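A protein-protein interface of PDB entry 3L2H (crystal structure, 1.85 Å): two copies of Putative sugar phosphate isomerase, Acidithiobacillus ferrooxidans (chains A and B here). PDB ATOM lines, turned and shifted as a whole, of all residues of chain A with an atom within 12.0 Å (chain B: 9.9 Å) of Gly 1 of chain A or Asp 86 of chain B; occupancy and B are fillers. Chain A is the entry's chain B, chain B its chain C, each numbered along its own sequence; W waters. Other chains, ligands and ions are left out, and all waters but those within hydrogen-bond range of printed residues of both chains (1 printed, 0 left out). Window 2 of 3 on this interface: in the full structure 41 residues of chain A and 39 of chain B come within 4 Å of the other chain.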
ATOM      1  N   GLY A   1       2.992   6.521 -10.890  1.00  0.00           N
ATOM      2  CA  GLY A   1       3.113   7.281  -9.582  1.00  0.00           C
ATOM      3  C   GLY A   1       3.318   6.370  -8.361  1.00  0.00           C
ATOM      4  O   GLY A   1       3.233   5.138  -8.485  1.00  0.00           O
ATOM      5  N   MET A   2       3.544   6.983  -7.190  1.00  0.00           N
ATOM      6  CA  MET A   2       3.893   6.260  -5.951  1.00  0.00           C
ATOM      7  C   MET A   2       2.858   5.270  -5.454  1.00  0.00           C
ATOM      8  O   MET A   2       3.199   4.245  -4.853  1.00  0.00           O
ATOM      9  CB  MET A   2       4.152   7.257  -4.819  1.00  0.00           C
ATOM     10  CG  MET A   2       4.387   6.574  -3.454  1.00  0.00           C
ATOM     11  SD  MET A   2       4.752   7.868  -1.995  1.00  0.00           S
ATOM     12  CE  MET A   2       4.744   6.595  -0.417  1.00  0.00           C
ATOM     13  N   ASP A   3       1.582   5.600  -5.686  1.00  0.00           N
ATOM     14  CA  ASP A   3       0.461   4.765  -5.209  1.00  0.00           C
ATOM     15  C   ASP A   3       0.323   3.412  -5.939  1.00  0.00           C
ATOM     16  O   ASP A   3      -0.460   2.577  -5.518  1.00  0.00           O
ATOM     17  CB  ASP A   3      -0.877   5.558  -5.249  1.00  0.00           C
ATOM     18  CG  ASP A   3      -1.191   6.206  -6.632  1.00  0.00           C
ATOM     19  OD1 ASP A   3      -0.411   6.038  -7.600  1.00  0.00           O
ATOM     20  OD2 ASP A   3      -2.225   6.934  -6.737  1.00  0.00           O
ATOM     21  N   THR A   4       1.102   3.237  -7.008  1.00  0.00           N
ATOM     22  CA  THR A   4       1.104   2.029  -7.823  1.00  0.00           C
ATOM     23  C   THR A   4       2.253   1.076  -7.470  1.00  0.00           C
ATOM     24  O   THR A   4       2.244  -0.084  -7.834  1.00  0.00           O
ATOM     25  CB  THR A   4       1.248   2.391  -9.305  1.00  0.00           C
ATOM     26  OG1 THR A   4       0.705   3.692  -9.551  1.00  0.00           O
ATOM     27  CG2 THR A   4       0.508   1.387 -10.138  1.00  0.00           C
ATOM     28  N   ARG A   5       3.239   1.575  -6.740  1.00  0.00           N
ATOM     29  CA  ARG A   5       4.383   0.748  -6.347  1.00  0.00           C
ATOM     30  C   ARG A   5       3.927  -0.488  -5.586  1.00  0.00           C
ATOM     31  O   ARG A   5       4.566  -1.544  -5.666  1.00  0.00           O
ATOM     32  CB  ARG A   5       5.392   1.570  -5.506  1.00  0.00           C
ATOM     33  CG  ARG A   5       6.534   0.739  -4.867  1.00  0.00           C
ATOM     34  CD  ARG A   5       7.470   0.155  -5.887  1.00  0.00           C
ATOM     35  NE  ARG A   5       8.527  -0.616  -5.216  1.00  0.00           N
ATOM     36  CZ  ARG A   5       8.377  -1.851  -4.730  1.00  0.00           C
ATOM     37  NH1 ARG A   5       7.219  -2.500  -4.861  1.00  0.00           N
ATOM     38  NH2 ARG A   5       9.403  -2.473  -4.133  1.00  0.00           N
ATOM     39  N   LYS A   6       2.811  -0.407  -4.875  1.00  0.00           N
ATOM     40  CA  LYS A   6       2.308  -1.544  -4.121  1.00  0.00           C
ATOM     41  C   LYS A   6       1.856  -2.712  -4.999  1.00  0.00           C
ATOM     42  O   LYS A   6       1.642  -3.794  -4.501  1.00  0.00           O
ATOM     43  CB  LYS A   6       1.164  -1.129  -3.222  1.00  0.00           C
ATOM     44  CG  LYS A   6      -0.008  -0.483  -3.960  1.00  0.00           C
ATOM     45  N   LEU A   7       1.720  -2.496  -6.305  1.00  0.00           N
ATOM     46  CA  LEU A   7       1.314  -3.587  -7.208  1.00  0.00           C
ATOM     47  C   LEU A   7       2.462  -4.511  -7.527  1.00  0.00           C
ATOM     48  O   LEU A   7       2.245  -5.649  -7.990  1.00  0.00           O
ATOM     49  CB  LEU A   7       0.723  -3.019  -8.493  1.00  0.00           C
ATOM     50  CG  LEU A   7      -0.526  -2.142  -8.301  1.00  0.00           C
ATOM     51  CD1 LEU A   7      -1.038  -1.712  -9.666  1.00  0.00           C
ATOM     52  CD2 LEU A   7      -1.617  -2.854  -7.545  1.00  0.00           C
ATOM     53  N   LEU A   8       3.694  -4.041  -7.276  1.00  0.00           N
ATOM     54  CA  LEU A   8       4.902  -4.857  -7.479  1.00  0.00           C
ATOM     55  C   LEU A   8       5.344  -5.416  -6.120  1.00  0.00           C
ATOM     56  O   LEU A   8       5.464  -4.659  -5.144  1.00  0.00           O
ATOM     57  CB  LEU A   8       5.995  -4.011  -8.065  1.00  0.00           C
ATOM     58  CG  LEU A   8       7.419  -4.565  -8.124  1.00  0.00           C
ATOM     59  CD1 LEU A   8       7.490  -5.779  -9.021  1.00  0.00           C
ATOM     60  CD2 LEU A   8       8.372  -3.442  -8.591  1.00  0.00           C
ATOM     61  N   TYR B  62       1.246  -0.873 -23.859  1.00  0.00           N
ATOM     62  CA  TYR B  62       0.869  -0.205 -22.606  1.00  0.00           C
ATOM     63  C   TYR B  62      -0.643  -0.145 -22.502  1.00  0.00           C
ATOM     64  O   TYR B  62      -1.318   0.448 -23.358  1.00  0.00           O
ATOM     65  CB  TYR B  62       1.441   1.186 -22.591  1.00  0.00           C
ATOM     66  CG  TYR B  62       1.377   1.961 -21.309  1.00  0.00           C
ATOM     67  CD1 TYR B  62       2.132   1.571 -20.187  1.00  0.00           C
ATOM     68  CD2 TYR B  62       0.671   3.154 -21.241  1.00  0.00           C
ATOM     69  CE1 TYR B  62       2.136   2.330 -19.033  1.00  0.00           C
ATOM     70  CE2 TYR B  62       0.701   3.941 -20.113  1.00  0.00           C
ATOM     71  CZ  TYR B  62       1.414   3.491 -18.983  1.00  0.00           C
ATOM     72  OH  TYR B  62       1.433   4.214 -17.823  1.00  0.00           O
ATOM     73  N   THR B  80      12.170  -4.302 -17.581  1.00  0.00           N
ATOM     74  CA  THR B  80      11.815  -3.004 -17.065  1.00  0.00           C
ATOM     75  C   THR B  80      10.308  -2.914 -17.145  1.00  0.00           C
ATOM     76  O   THR B  80       9.734  -3.051 -18.202  1.00  0.00           O
ATOM     77  CB  THR B  80      12.478  -1.896 -17.882  1.00  0.00           C
ATOM     78  OG1 THR B  80      13.875  -2.016 -17.718  1.00  0.00           O
ATOM     79  CG2 THR B  80      12.069  -0.496 -17.395  1.00  0.00           C
ATOM     80  N   LEU B  81       9.680  -2.772 -16.000  1.00  0.00           N
ATOM     81  CA  LEU B  81       8.242  -2.590 -15.899  1.00  0.00           C
ATOM     82  C   LEU B  81       7.945  -1.095 -15.955  1.00  0.00           C
ATOM     83  O   LEU B  81       8.513  -0.314 -15.183  1.00  0.00           O
ATOM     84  CB  LEU B  81       7.779  -3.137 -14.575  1.00  0.00           C
ATOM     85  CG  LEU B  81       6.353  -2.857 -14.095  1.00  0.00           C
ATOM     86  CD1 LEU B  81       5.288  -3.470 -15.048  1.00  0.00           C
ATOM     87  CD2 LEU B  81       6.181  -3.348 -12.646  1.00  0.00           C
ATOM     88  N   THR B  82       7.114  -0.687 -16.898  1.00  0.00           N
ATOM     89  CA  THR B  82       6.583   0.669 -16.931  1.00  0.00           C
ATOM     90  C   THR B  82       5.167   0.571 -16.422  1.00  0.00           C
ATOM     91  O   THR B  82       4.367  -0.161 -16.957  1.00  0.00           O
ATOM     92  CB  THR B  82       6.613   1.297 -18.338  1.00  0.00           C
ATOM     93  OG1 THR B  82       7.957   1.368 -18.769  1.00  0.00           O
ATOM     94  CG2 THR B  82       6.073   2.727 -18.360  1.00  0.00           C
ATOM     95  N   MET B  83       4.875   1.322 -15.373  1.00  0.00           N
ATOM     96  CA  MET B  83       3.564   1.317 -14.758  1.00  0.00           C
ATOM     97  C   MET B  83       3.211   2.724 -14.337  1.00  0.00           C
ATOM     98  O   MET B  83       3.930   3.334 -13.550  1.00  0.00           O
ATOM     99  CB  MET B  83       3.635   0.344 -13.580  1.00  0.00           C
ATOM    100  CG  MET B  83       2.407   0.137 -12.810  1.00  0.00           C
ATOM    101  SD  MET B  83       2.695  -1.416 -11.573  1.00  0.00           S
ATOM    102  CE  MET B  83       4.137  -0.776 -10.526  1.00  0.00           C
ATOM    103  N   GLU B  84       2.107   3.252 -14.865  1.00  0.00           N
ATOM    104  CA  GLU B  84       1.680   4.646 -14.631  1.00  0.00           C
ATOM    105  C   GLU B  84       2.855   5.599 -14.805  1.00  0.00           C
ATOM    106  O   GLU B  84       3.117   6.450 -13.950  1.00  0.00           O
ATOM    107  CB  GLU B  84       0.996   4.788 -13.242  1.00  0.00           C
ATOM    108  CG  GLU B  84      -0.357   4.048 -13.214  1.00  0.00           C
ATOM    109  CD  GLU B  84      -1.370   4.665 -14.137  1.00  0.00           C
ATOM    110  OE1 GLU B  84      -1.560   5.869 -14.018  1.00  0.00           O
ATOM    111  OE2 GLU B  84      -1.954   3.986 -15.010  1.00  0.00           O
ATOM    112  N   ASN B  85       3.576   5.423 -15.921  1.00  0.00           N
ATOM    113  CA  ASN B  85       4.662   6.309 -16.328  1.00  0.00           C
ATOM    114  C   ASN B  85       5.934   6.275 -15.466  1.00  0.00           C
ATOM    115  O   ASN B  85       6.829   7.111 -15.652  1.00  0.00           O
ATOM    116  CB  ASN B  85       4.130   7.734 -16.441  1.00  0.00           C
ATOM    117  CG  ASN B  85       3.151   7.862 -17.589  1.00  0.00           C
ATOM    118  OD1 ASN B  85       3.271   7.128 -18.605  1.00  0.00           O
ATOM    119  ND2 ASN B  85       2.159   8.732 -17.441  1.00  0.00           N
ATOM    120  N   ASP B  86       6.033   5.322 -14.564  1.00  0.00           N
ATOM    121  CA  ASP B  86       7.269   5.116 -13.832  1.00  0.00           C
ATOM    122  C   ASP B  86       7.881   3.791 -14.252  1.00  0.00           C
ATOM    123  O   ASP B  86       7.157   2.866 -14.587  1.00  0.00           O
ATOM    124  CB  ASP B  86       7.006   5.144 -12.349  1.00  0.00           C
ATOM    125  CG  ASP B  86       6.663   6.545 -11.840  1.00  0.00           C
ATOM    126  OD1 ASP B  86       7.405   7.484 -12.048  1.00  0.00           O
ATOM    127  OD2 ASP B  86       5.687   6.708 -11.131  1.00  0.00           O
ATOM    128  N   GLN B  87       9.212   3.725 -14.237  1.00  0.00           N
ATOM    129  CA  GLN B  87       9.944   2.552 -14.603  1.00  0.00           C
ATOM    130  C   GLN B  87      10.552   1.879 -13.381  1.00  0.00           C
ATOM    131  O   GLN B  87      11.159   2.544 -12.484  1.00  0.00           O
ATOM    132  CB  GLN B  87      11.043   2.939 -15.602  1.00  0.00           C
ATOM    133  CG  GLN B  87      10.429   3.371 -16.932  1.00  0.00           C
ATOM    134  CD  GLN B  87      11.469   3.566 -17.990  1.00  0.00           C
ATOM    135  OE1 GLN B  87      12.622   3.745 -17.688  1.00  0.00           O
ATOM    136  NE2 GLN B  87      11.057   3.560 -19.245  1.00  0.00           N
ATOM    137  N   TYR B  88      10.423   0.555 -13.373  1.00  0.00           N
ATOM    138  CA  TYR B  88      10.934  -0.277 -12.287  1.00  0.00           C
ATOM    139  C   TYR B  88      11.708  -1.481 -12.855  1.00  0.00           C
ATOM    140  O   TYR B  88      11.233  -2.167 -13.745  1.00  0.00           O
ATOM    141  CB  TYR B  88       9.797  -0.809 -11.409  1.00  0.00           C
ATOM    142  CG  TYR B  88       8.844   0.225 -10.814  1.00  0.00           C
ATOM    143  CD1 TYR B  88       7.784   0.664 -11.550  1.00  0.00           C
ATOM    144  CD2 TYR B  88       9.046   0.789  -9.555  1.00  0.00           C
ATOM    145  CE1 TYR B  88       6.905   1.603 -11.087  1.00  0.00           C
ATOM    146  CE2 TYR B  88       8.138   1.764  -9.053  1.00  0.00           C
ATOM    147  CZ  TYR B  88       7.065   2.144  -9.834  1.00  0.00           C
ATOM    148  OH  TYR B  88       6.091   3.117  -9.457  1.00  0.00           O
ATOM    149  N   PRO B  89      12.843  -1.814 -12.269  1.00  0.00           N
ATOM    150  CA  PRO B  89      13.539  -3.011 -12.718  1.00  0.00           C
ATOM    151  C   PRO B  89      12.785  -4.230 -12.226  1.00  0.00           C
ATOM    152  O   PRO B  89      12.267  -4.191 -11.107  1.00  0.00           O
ATOM    153  CB  PRO B  89      14.870  -2.901 -12.000  1.00  0.00           C
ATOM    154  CG  PRO B  89      14.447  -2.302 -10.604  1.00  0.00           C
ATOM    155  CD  PRO B  89      13.459  -1.219 -11.062  1.00  0.00           C
ATOM    156  N   ILE B  90      12.647  -5.283 -13.053  1.00  0.00           N
ATOM    157  CA  ILE B  90      12.025  -6.543 -12.561  1.00  0.00           C
ATOM    158  C   ILE B  90      13.014  -7.682 -12.859  1.00  0.00           C
ATOM    159  O   ILE B  90      13.839  -7.584 -13.762  1.00  0.00           O
ATOM    160  CB  ILE B  90      10.617  -6.832 -13.091  1.00  0.00           C
ATOM    161  CG1 ILE B  90      10.585  -6.907 -14.627  1.00  0.00           C
ATOM    162  CG2 ILE B  90       9.588  -5.771 -12.536  1.00  0.00           C
ATOM    163  CD1 ILE B  90       9.200  -7.387 -15.211  1.00  0.00           C
ATOM    164  N   VAL B  96       3.991  -8.996 -10.110  1.00  0.00           N
ATOM    165  CA  VAL B  96       3.228  -7.759 -10.291  1.00  0.00           C
ATOM    166  C   VAL B  96       1.820  -8.136 -10.646  1.00  0.00           C
ATOM    167  O   VAL B  96       1.602  -9.020 -11.503  1.00  0.00           O
ATOM    168  CB  VAL B  96       3.899  -6.773 -11.329  1.00  0.00           C
ATOM    169  CG1 VAL B  96       4.004  -7.371 -12.634  1.00  0.00           C
ATOM    170  CG2 VAL B  96       3.145  -5.441 -11.415  1.00  0.00           C
ATOM    171  N   PHE B  98      -2.357  -6.793 -11.288  1.00  0.00           N
ATOM    172  CA  PHE B  98      -3.197  -5.682 -11.712  1.00  0.00           C
ATOM    173  C   PHE B  98      -4.684  -5.883 -11.454  1.00  0.00           C
ATOM    174  O   PHE B  98      -5.403  -6.497 -12.305  1.00  0.00           O
ATOM    175  CB  PHE B  98      -2.961  -5.405 -13.208  1.00  0.00           C
ATOM    176  CG  PHE B  98      -1.546  -5.042 -13.522  1.00  0.00           C
ATOM    177  CD1 PHE B  98      -1.109  -3.729 -13.373  1.00  0.00           C
ATOM    178  CD2 PHE B  98      -0.620  -6.020 -13.884  1.00  0.00           C
ATOM    179  CE1 PHE B  98       0.231  -3.401 -13.614  1.00  0.00           C
ATOM    180  CE2 PHE B  98       0.728  -5.671 -14.151  1.00  0.00           C
ATOM    181  CZ  PHE B  98       1.142  -4.373 -13.980  1.00  0.00           C
ATOM    182  N   ALA B 102      -6.410  -0.388 -12.034  1.00  0.00           N
ATOM    183  CA  ALA B 102      -5.425   0.076 -11.074  1.00  0.00           C
ATOM    184  C   ALA B 102      -4.301   0.843 -11.759  1.00  0.00           C
ATOM    185  O   ALA B 102      -3.898   1.916 -11.298  1.00  0.00           O
ATOM    186  CB  ALA B 102      -4.852  -1.117 -10.249  1.00  0.00           C
ATOM    187  N   ALA B 103      -3.773   0.297 -12.846  1.00  0.00           N
ATOM    188  CA  ALA B 103      -2.573   0.872 -13.440  1.00  0.00           C
ATOM    189  C   ALA B 103      -2.327   0.328 -14.827  1.00  0.00           C
ATOM    190  O   ALA B 103      -2.491  -0.864 -15.063  1.00  0.00           O
ATOM    191  CB  ALA B 103      -1.336   0.606 -12.552  1.00  0.00           C
ATOM    192  N   ALA B 104      -2.021   1.240 -15.737  1.00  0.00           N
ATOM    193  CA  ALA B 104      -1.567   0.908 -17.078  1.00  0.00           C
ATOM    194  C   ALA B 104      -0.123   0.425 -16.957  1.00  0.00           C
ATOM    195  O   ALA B 104       0.636   0.932 -16.140  1.00  0.00           O
ATOM    196  CB  ALA B 104      -1.628   2.107 -18.010  1.00  0.00           C
ATOM    197  N   HIS B 105       0.237  -0.583 -17.720  1.00  0.00           N
ATOM    198  CA  HIS B 105       1.601  -1.062 -17.692  1.00  0.00           C
ATOM    199  C   HIS B 105       2.027  -1.687 -18.999  1.00  0.00           C
ATOM    200  O   HIS B 105       1.176  -2.021 -19.854  1.00  0.00           O
ATOM    201  CB  HIS B 105       1.762  -2.129 -16.621  1.00  0.00           C
ATOM    202  CG  HIS B 105       1.576  -3.538 -17.118  1.00  0.00           C
ATOM    203  ND1 HIS B 105       0.335  -4.117 -17.234  1.00  0.00           N
ATOM    204  CD2 HIS B 105       2.461  -4.504 -17.451  1.00  0.00           C
ATOM    205  CE1 HIS B 105       0.454  -5.347 -17.698  1.00  0.00           C
ATOM    206  NE2 HIS B 105       1.737  -5.622 -17.823  1.00  0.00           N
ATOM    207  N   SER B 106       3.353  -1.837 -19.134  1.00  0.00           N
ATOM    208  CA  SER B 106       3.961  -2.687 -20.146  1.00  0.00           C
ATOM    209  C   SER B 106       5.326  -3.128 -19.601  1.00  0.00           C
ATOM    210  O   SER B 106       5.895  -2.461 -18.731  1.00  0.00           O
ATOM    211  CB  SER B 106       4.105  -1.988 -21.511  1.00  0.00           C
ATOM    212  OG  SER B 106       4.973  -0.886 -21.365  1.00  0.00           O
ATOM    213  N   ILE B 107       5.836  -4.230 -20.119  1.00  0.00           N
ATOM    214  CA  ILE B 107       7.151  -4.736 -19.771  1.00  0.00           C
ATOM    215  C   ILE B 107       8.050  -4.796 -20.999  1.00  0.00           C
ATOM    216  O   ILE B 107       7.643  -5.211 -22.093  1.00  0.00           O
ATOM    217  CB  ILE B 107       7.099  -6.109 -19.138  1.00  0.00           C
ATOM    218  CG1 ILE B 107       6.442  -6.042 -17.764  1.00  0.00           C
ATOM    219  CG2 ILE B 107       8.561  -6.720 -19.002  1.00  0.00           C
ATOM    220  CD1 ILE B 107       5.871  -7.374 -17.265  1.00  0.00           C
ATOM    221  N   SER B 108       9.265  -4.343 -20.809  1.00  0.00           N
ATOM    222  CA  SER B 108      10.253  -4.338 -21.823  1.00  0.00           C
ATOM    223  C   SER B 108      11.484  -5.144 -21.374  1.00  0.00           C
ATOM    224  O   SER B 108      11.864  -5.110 -20.188  1.00  0.00           O
ATOM    225  CB  SER B 108      10.637  -2.895 -22.072  1.00  0.00           C
ATOM    226  OG  SER B 108      11.491  -2.852 -23.164  1.00  0.00           O
HETATM  227  O   HOH W   1       3.854   3.404 -10.857  1.00  0.00           O
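O of Glu 84 of chain B sits at hydrogen-bond distance from N of Gly 1 of chain A, at 3.1 Å. The backbone NH (N) of Gly 1 of chain A sits at hydrogen-bond distance from the side-chain carboxylate (OD2) of Asp 86 of chain B.
The backbone carbonyl oxygen (O) of Gly 1 of chain A is in hydrogen-bond range of the side-chain hydroxyl (OG1) of Thr 4 of chain A, 3.1 Å away. OD1 of Asp 3 of chain A lies within hydrogen-bond range of OG1 of Thr 4 of chain A (3.2 Å). NH1 of Arg 5 of chain A is in hydrogen-bond range of O of Leu 8 of chain A (2.8 Å). OH of Tyr 62 of chain B sits at hydrogen-bond distance from N of Glu 84 of chain B, at 3.2 Å. The backbone carbonyl oxygen (O) of Leu 81 of chain B lies within hydrogen-bond range of the backbone NH (N) of Tyr 88 of chain B, at 2.8 Å. OE2 of Glu 84 of chain B lies within hydrogen-bond range of N of Ala 104 of chain B, at 2.8 Å.
Among the printed residues, merely in contact across the chains: Gly 1 of chain A with Tyr 88 of chain B (3.6 Å), Thr 4 of chain A with Met 83 of chain B (3.4 Å), Thr 4 of chain A with Glu 84 of chain B (3.8 Å), Thr 4 of chain A with Ala 103 of chain B (3.1 Å), Arg 5 of chain A with Tyr 88 of chain B (3.6 Å), Leu 7 of chain A with Met 83 of chain B (3.99 Å), Leu 7 of chain A with Val 96 of chain B (3.3 Å), Leu 7 of chain A with Ala 102 of chain B (3.9 Å) and Leu 7 of chain A with Ala 103 of chain B (3.7 Å).
Gly 1 of chain A touches three residues of chain B. Of chain A, only Gly 1 comes within 4 Å of Asp 86 of chain B. No residue of chain A comes within 4 Å of Leu 81 of chain B. No residue of chain A comes within 4 Å of Gln 87 of chain B. Of chain A, only Gly 1 and Arg 5 come within 4 Å of Tyr 88 of chain B. Printed residues of chain A within 4 Å of Ala 103 of chain B: Thr 4 and Leu 7. Of the printed residues of chain B, Arg 5 of chain A touches Tyr 88. Of the printed residues of chain A, Ala 102 of chain B touches Leu 7. Ile 107 of chain B touches none of the printed residues of chain A. The nearest residue of chain B that does not touch Gly 1 of chain A is Met 83 of chain B (4.3 Å). The nearest residue of chain A that does not touch Asp 86 of chain B is Met 2 of chain A (4.5 Å).
Of the 21 printed residues of chain B, 7 touch a printed residue of chain A. Of the 8 printed residues of chain A, 4 touch a printed residue of chain B. Printed residues of chain A that touch a printed residue of chain B: Gly 1, Thr 4, Arg 5 and Leu 7. Hydrophobic or aromatic side chains of chain A that line the printed part of chain B: Leu 7. Among the printed residues, no Asp or Glu carboxylate lies within 4 Å of a Lys or Arg side-chain nitrogen of the other chain.
No position is printed for both chains.
Water W1 lies within hydrogen-bond range of the side-chain hydroxyl of Tyr 88 of chain B, the backbone carbonyl oxygen of Met 83 of chain B, the backbone carbonyl oxygen of Gly 1 of chain A and the side-chain hydroxyl of Thr 4 of chain A.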
